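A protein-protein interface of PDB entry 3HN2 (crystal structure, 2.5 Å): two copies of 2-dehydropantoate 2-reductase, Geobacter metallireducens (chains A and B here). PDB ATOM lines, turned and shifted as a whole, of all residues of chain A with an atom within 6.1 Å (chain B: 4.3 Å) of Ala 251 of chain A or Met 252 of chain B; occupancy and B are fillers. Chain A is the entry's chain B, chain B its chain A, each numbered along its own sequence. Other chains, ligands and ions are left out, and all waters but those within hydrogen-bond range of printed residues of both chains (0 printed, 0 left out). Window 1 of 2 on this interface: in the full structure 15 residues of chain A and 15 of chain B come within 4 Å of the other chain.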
ATOM      1  N   LEU A 141      25.809  10.894  -1.401  1.00  0.00           N
ATOM      2  CA  LEU A 141      25.173   9.582  -1.336  1.00  0.00           C
ATOM      3  C   LEU A 141      24.929   9.098   0.089  1.00  0.00           C
ATOM      4  O   LEU A 141      24.109   8.204   0.314  1.00  0.00           O
ATOM      5  CB  LEU A 141      25.999   8.542  -2.102  1.00  0.00           C
ATOM      6  CG  LEU A 141      26.178   8.666  -3.618  1.00  0.00           C
ATOM      7  CD1 LEU A 141      26.790   7.384  -4.168  1.00  0.00           C
ATOM      8  CD2 LEU A 141      24.868   8.994  -4.334  1.00  0.00           C
ATOM      9  N   LEU A 246      33.366  -3.916  10.871  1.00  0.00           N
ATOM     10  CA  LEU A 246      32.887  -5.014  10.034  1.00  0.00           C
ATOM     11  C   LEU A 246      31.368  -4.952   9.893  1.00  0.00           C
ATOM     12  O   LEU A 246      30.837  -5.087   8.791  1.00  0.00           O
ATOM     13  CB  LEU A 246      33.311  -6.357  10.631  1.00  0.00           C
ATOM     14  CG  LEU A 246      33.908  -7.427   9.717  1.00  0.00           C
ATOM     15  CD1 LEU A 246      35.215  -6.953   9.094  1.00  0.00           C
ATOM     16  CD2 LEU A 246      34.139  -8.705  10.505  1.00  0.00           C
ATOM     17  N   GLU A 247      30.683  -4.732  11.016  1.00  0.00           N
ATOM     18  CA  GLU A 247      29.225  -4.577  11.047  1.00  0.00           C
ATOM     19  C   GLU A 247      28.759  -3.244  10.457  1.00  0.00           C
ATOM     20  O   GLU A 247      27.644  -3.144   9.949  1.00  0.00           O
ATOM     21  CB  GLU A 247      28.707  -4.718  12.479  1.00  0.00           C
ATOM     22  CG  GLU A 247      28.761  -6.142  13.019  1.00  0.00           C
ATOM     23  CD  GLU A 247      28.839  -6.205  14.536  1.00  0.00           C
ATOM     24  OE1 GLU A 247      29.149  -7.296  15.060  1.00  0.00           O
ATOM     25  OE2 GLU A 247      28.599  -5.172  15.203  1.00  0.00           O
ATOM     26  N   PHE A 248      29.624  -2.235  10.542  1.00  0.00           N
ATOM     27  CA  PHE A 248      29.386  -0.896   9.995  1.00  0.00           C
ATOM     28  C   PHE A 248      29.254  -0.934   8.474  1.00  0.00           C
ATOM     29  O   PHE A 248      28.306  -0.386   7.917  1.00  0.00           O
ATOM     30  CB  PHE A 248      30.539   0.026  10.419  1.00  0.00           C
ATOM     31  CG  PHE A 248      30.447   1.434   9.893  1.00  0.00           C
ATOM     32  CD1 PHE A 248      29.608   2.368  10.498  1.00  0.00           C
ATOM     33  CD2 PHE A 248      31.242   1.840   8.822  1.00  0.00           C
ATOM     34  CE1 PHE A 248      29.541   3.677  10.025  1.00  0.00           C
ATOM     35  CE2 PHE A 248      31.184   3.145   8.345  1.00  0.00           C
ATOM     36  CZ  PHE A 248      30.331   4.067   8.946  1.00  0.00           C
ATOM     37  N   THR A 249      30.205  -1.604   7.823  1.00  0.00           N
ATOM     38  CA  THR A 249      30.280  -1.707   6.363  1.00  0.00           C
ATOM     39  C   THR A 249      29.186  -2.619   5.806  1.00  0.00           C
ATOM     40  O   THR A 249      28.811  -2.514   4.637  1.00  0.00           O
ATOM     41  CB  THR A 249      31.664  -2.252   5.916  1.00  0.00           C
ATOM     42  OG1 THR A 249      32.676  -1.801   6.822  1.00  0.00           O
ATOM     43  CG2 THR A 249      32.012  -1.791   4.502  1.00  0.00           C
ATOM     44  N   ASP A 250      28.670  -3.496   6.664  1.00  0.00           N
ATOM     45  CA  ASP A 250      27.641  -4.474   6.308  1.00  0.00           C
ATOM     46  C   ASP A 250      26.289  -3.828   5.970  1.00  0.00           C
ATOM     47  O   ASP A 250      25.411  -4.475   5.389  1.00  0.00           O
ATOM     48  CB  ASP A 250      27.474  -5.475   7.458  1.00  0.00           C
ATOM     49  CG  ASP A 250      27.358  -6.914   6.981  1.00  0.00           C
ATOM     50  OD1 ASP A 250      27.972  -7.800   7.618  1.00  0.00           O
ATOM     51  OD2 ASP A 250      26.658  -7.166   5.977  1.00  0.00           O
ATOM     52  N   ALA A 251      26.131  -2.555   6.334  1.00  0.00           N
ATOM     53  CA  ALA A 251      24.916  -1.805   6.034  1.00  0.00           C
ATOM     54  C   ALA A 251      25.155  -0.654   5.048  1.00  0.00           C
ATOM     55  O   ALA A 251      24.388   0.312   5.010  1.00  0.00           O
ATOM     56  CB  ALA A 251      24.289  -1.292   7.316  1.00  0.00           C
ATOM     57  N   MET A 252      26.214  -0.770   4.252  1.00  0.00           N
ATOM     58  CA  MET A 252      26.535   0.216   3.217  1.00  0.00           C
ATOM     59  C   MET A 252      26.023  -0.209   1.847  1.00  0.00           C
ATOM     60  O   MET A 252      26.114   0.559   0.884  1.00  0.00           O
ATOM     61  CB  MET A 252      28.044   0.440   3.137  1.00  0.00           C
ATOM     62  CG  MET A 252      28.567   1.524   4.052  1.00  0.00           C
ATOM     63  SD  MET A 252      30.357   1.603   3.985  1.00  0.00           S
ATOM     64  CE  MET A 252      30.672   3.186   4.747  1.00  0.00           C
ATOM     65  N   GLY A 253      25.490  -1.429   1.770  1.00  0.00           N
ATOM     66  CA  GLY A 253      25.010  -2.002   0.514  1.00  0.00           C
ATOM     67  C   GLY A 253      26.113  -2.218  -0.510  1.00  0.00           C
ATOM     68  O   GLY A 253      27.193  -2.720  -0.180  1.00  0.00           O
ATOM     69  N   PHE B 127      19.094  -9.259  10.590  1.00  0.00           N
ATOM     70  CA  PHE B 127      19.158  -7.882  10.109  1.00  0.00           C
ATOM     71  C   PHE B 127      19.351  -7.860   8.600  1.00  0.00           C
ATOM     72  O   PHE B 127      20.418  -8.207   8.096  1.00  0.00           O
ATOM     73  CB  PHE B 127      20.258  -7.087  10.816  1.00  0.00           C
ATOM     74  CG  PHE B 127      20.036  -5.600  10.784  1.00  0.00           C
ATOM     75  CD1 PHE B 127      19.297  -4.975  11.789  1.00  0.00           C
ATOM     76  CD2 PHE B 127      20.551  -4.824   9.749  1.00  0.00           C
ATOM     77  CE1 PHE B 127      19.079  -3.597  11.765  1.00  0.00           C
ATOM     78  CE2 PHE B 127      20.337  -3.450   9.717  1.00  0.00           C
ATOM     79  CZ  PHE B 127      19.601  -2.835  10.728  1.00  0.00           C
ATOM     80  N   TRP B 189      17.250  -0.150  17.673  1.00  0.00           N
ATOM     81  CA  TRP B 189      17.257   0.384  16.319  1.00  0.00           C
ATOM     82  C   TRP B 189      15.854   0.480  15.730  1.00  0.00           C
ATOM     83  O   TRP B 189      15.504   1.495  15.097  1.00  0.00           O
ATOM     84  CB  TRP B 189      18.148  -0.455  15.393  1.00  0.00           C
ATOM     85  CG  TRP B 189      18.404   0.255  14.116  1.00  0.00           C
ATOM     86  CD1 TRP B 189      19.422   1.138  13.856  1.00  0.00           C
ATOM     87  CD2 TRP B 189      17.609   0.196  12.925  1.00  0.00           C
ATOM     88  NE1 TRP B 189      19.318   1.606  12.572  1.00  0.00           N
ATOM     89  CE2 TRP B 189      18.212   1.062  11.978  1.00  0.00           C
ATOM     90  CE3 TRP B 189      16.450  -0.506  12.563  1.00  0.00           C
ATOM     91  CZ2 TRP B 189      17.697   1.239  10.691  1.00  0.00           C
ATOM     92  CZ3 TRP B 189      15.925  -0.326  11.277  1.00  0.00           C
ATOM     93  CH2 TRP B 189      16.554   0.543  10.358  1.00  0.00           C
ATOM     94  N   PHE B 248      25.851   3.895  12.997  1.00  0.00           N
ATOM     95  CA  PHE B 248      25.563   2.732  12.145  1.00  0.00           C
ATOM     96  C   PHE B 248      24.529   3.061  11.076  1.00  0.00           C
ATOM     97  O   PHE B 248      24.717   2.723   9.909  1.00  0.00           O
ATOM     98  CB  PHE B 248      25.097   1.550  13.010  1.00  0.00           C
ATOM     99  CG  PHE B 248      24.548   0.380  12.235  1.00  0.00           C
ATOM    100  CD1 PHE B 248      25.405  -0.536  11.631  1.00  0.00           C
ATOM    101  CD2 PHE B 248      23.173   0.170  12.150  1.00  0.00           C
ATOM    102  CE1 PHE B 248      24.901  -1.623  10.929  1.00  0.00           C
ATOM    103  CE2 PHE B 248      22.659  -0.913  11.448  1.00  0.00           C
ATOM    104  CZ  PHE B 248      23.525  -1.815  10.839  1.00  0.00           C
ATOM    105  N   THR B 249      23.451   3.731  11.484  1.00  0.00           N
ATOM    106  CA  THR B 249      22.346   4.090  10.589  1.00  0.00           C
ATOM    107  C   THR B 249      22.773   5.185   9.602  1.00  0.00           C
ATOM    108  O   THR B 249      22.175   5.340   8.541  1.00  0.00           O
ATOM    109  CB  THR B 249      21.083   4.525  11.394  1.00  0.00           C
ATOM    110  OG1 THR B 249      21.052   3.836  12.645  1.00  0.00           O
ATOM    111  CG2 THR B 249      19.800   4.187  10.662  1.00  0.00           C
ATOM    112  N   ASP B 250      23.835   5.910   9.951  1.00  0.00           N
ATOM    113  CA  ASP B 250      24.382   6.992   9.134  1.00  0.00           C
ATOM    114  C   ASP B 250      25.148   6.483   7.901  1.00  0.00           C
ATOM    115  O   ASP B 250      25.497   7.264   7.011  1.00  0.00           O
ATOM    116  CB  ASP B 250      25.302   7.860   9.998  1.00  0.00           C
ATOM    117  CG  ASP B 250      25.133   9.348   9.734  1.00  0.00           C
ATOM    118  OD1 ASP B 250      25.372  10.141  10.671  1.00  0.00           O
ATOM    119  OD2 ASP B 250      24.761   9.731   8.602  1.00  0.00           O
ATOM    120  N   ALA B 251      25.408   5.177   7.856  1.00  0.00           N
ATOM    121  CA  ALA B 251      26.090   4.537   6.729  1.00  0.00           C
ATOM    122  C   ALA B 251      25.104   3.862   5.773  1.00  0.00           C
ATOM    123  O   ALA B 251      25.502   3.099   4.888  1.00  0.00           O
ATOM    124  CB  ALA B 251      27.099   3.515   7.245  1.00  0.00           C
ATOM    125  N   MET B 252      23.819   4.150   5.958  1.00  0.00           N
ATOM    126  CA  MET B 252      22.761   3.460   5.237  1.00  0.00           C
ATOM    127  C   MET B 252      22.194   4.308   4.129  1.00  0.00           C
ATOM    128  O   MET B 252      21.356   3.834   3.361  1.00  0.00           O
ATOM    129  CB  MET B 252      21.631   3.079   6.190  1.00  0.00           C
ATOM    130  CG  MET B 252      21.880   1.836   7.009  1.00  0.00           C
ATOM    131  SD  MET B 252      20.535   1.671   8.179  1.00  0.00           S
ATOM    132  CE  MET B 252      20.359  -0.114   8.309  1.00  0.00           C
ATOM    133  N   GLY B 253      22.646   5.561   4.060  1.00  0.00           N
ATOM    134  CA  GLY B 253      22.163   6.528   3.079  1.00  0.00           C
ATOM    135  C   GLY B 253      20.660   6.725   3.157  1.00  0.00           C
ATOM    136  O   GLY B 253      20.107   6.932   4.239  1.00  0.00           O
ATOM    137  N   GLU B 254      20.008   6.607   2.004  1.00  0.00           N
ATOM    138  CA  GLU B 254      18.586   6.893   1.848  1.00  0.00           C
ATOM    139  C   GLU B 254      17.725   5.630   2.023  1.00  0.00           C
ATOM    140  O   GLU B 254      17.013   5.213   1.106  1.00  0.00           O
ATOM    141  CB  GLU B 254      18.354   7.545   0.478  1.00  0.00           C
ATOM    142  CG  GLU B 254      17.098   8.402   0.370  1.00  0.00           C
ATOM    143  CD  GLU B 254      16.890   8.982  -1.022  1.00  0.00           C
ATOM    144  OE1 GLU B 254      16.246  10.046  -1.127  1.00  0.00           O
ATOM    145  OE2 GLU B 254      17.364   8.381  -2.011  1.00  0.00           O
ATOM    146  N   TYR B 255      17.781   5.032   3.210  1.00  0.00           N
ATOM    147  CA  TYR B 255      17.125   3.741   3.449  1.00  0.00           C
ATOM    148  C   TYR B 255      15.730   3.861   4.059  1.00  0.00           C
ATOM    149  O   TYR B 255      15.534   4.538   5.067  1.00  0.00           O
ATOM    150  CB  TYR B 255      18.010   2.840   4.312  1.00  0.00           C
ATOM    151  CG  TYR B 255      17.360   1.536   4.718  1.00  0.00           C
ATOM    152  CD1 TYR B 255      17.057   1.277   6.053  1.00  0.00           C
ATOM    153  CD2 TYR B 255      17.044   0.561   3.768  1.00  0.00           C
ATOM    154  CE1 TYR B 255      16.458   0.089   6.434  1.00  0.00           C
ATOM    155  CE2 TYR B 255      16.439  -0.634   4.141  1.00  0.00           C
ATOM    156  CZ  TYR B 255      16.150  -0.863   5.476  1.00  0.00           C
ATOM    157  OH  TYR B 255      15.559  -2.043   5.864  1.00  0.00           O
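O of Ala 251 of chain B lies close to O of Ala 251 of chain A, at 3.0 Å.
Among the printed residues, pairs that only touch across the chains: Glu 247 of chain A with Phe 248 of chain B, Met 252 of chain A with Ala 251 of chain B, Ala 251 of chain A with Met 252 of chain B, Ala 251 of chain A with Phe 248 of chain B, Phe 248 of chain A with Ala 251 of chain B and Leu 141 of chain A with Gly 253 of chain B.
Of chain B, only Phe 248 (3.6 Å), Ala 251 (3.0 Å) and Met 252 (3.6 Å) come within 4 Å of Ala 251 of chain A.
Of chain A, only Ala 251 comes within 4 Å of Met 252 of chain B.
Printed residues of chain B within 4 Å of Glu 247 of chain A: Phe 248 (3.3 Å).
Printed residues of chain B within 4 Å of Met 252 of chain A: Ala 251 (3.5 Å).
Glu 254 of chain B touches none of the printed residues of chain A.
The nearest printed residue of chain B that does not touch Ala 251 of chain A is Phe 127 of chain B (5.1 Å).
Of the 10 printed residues of chain B, 4 touch a printed residue of chain A.
Hydrophobic or aromatic side chains of chain B that line the printed part of chain A: Phe 248, Ala 251 and Met 252.
Among the printed residues, no Asp or Glu carboxylate lies within 4 Å of a Lys or Arg side-chain nitrogen of the other chain.
Phe 248 of chain A touches Ala 251 of chain B, and with the chains exchanged Ala 251 of chain A touches Phe 248 of chain B.
Ala 251 of chain A touches its own counterpart, Ala 251 of chain B.
Ala 251 of chain A touches Met 252 of chain B, and with the chains exchanged Met 252 of chain A touches Ala 251 of chain B.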
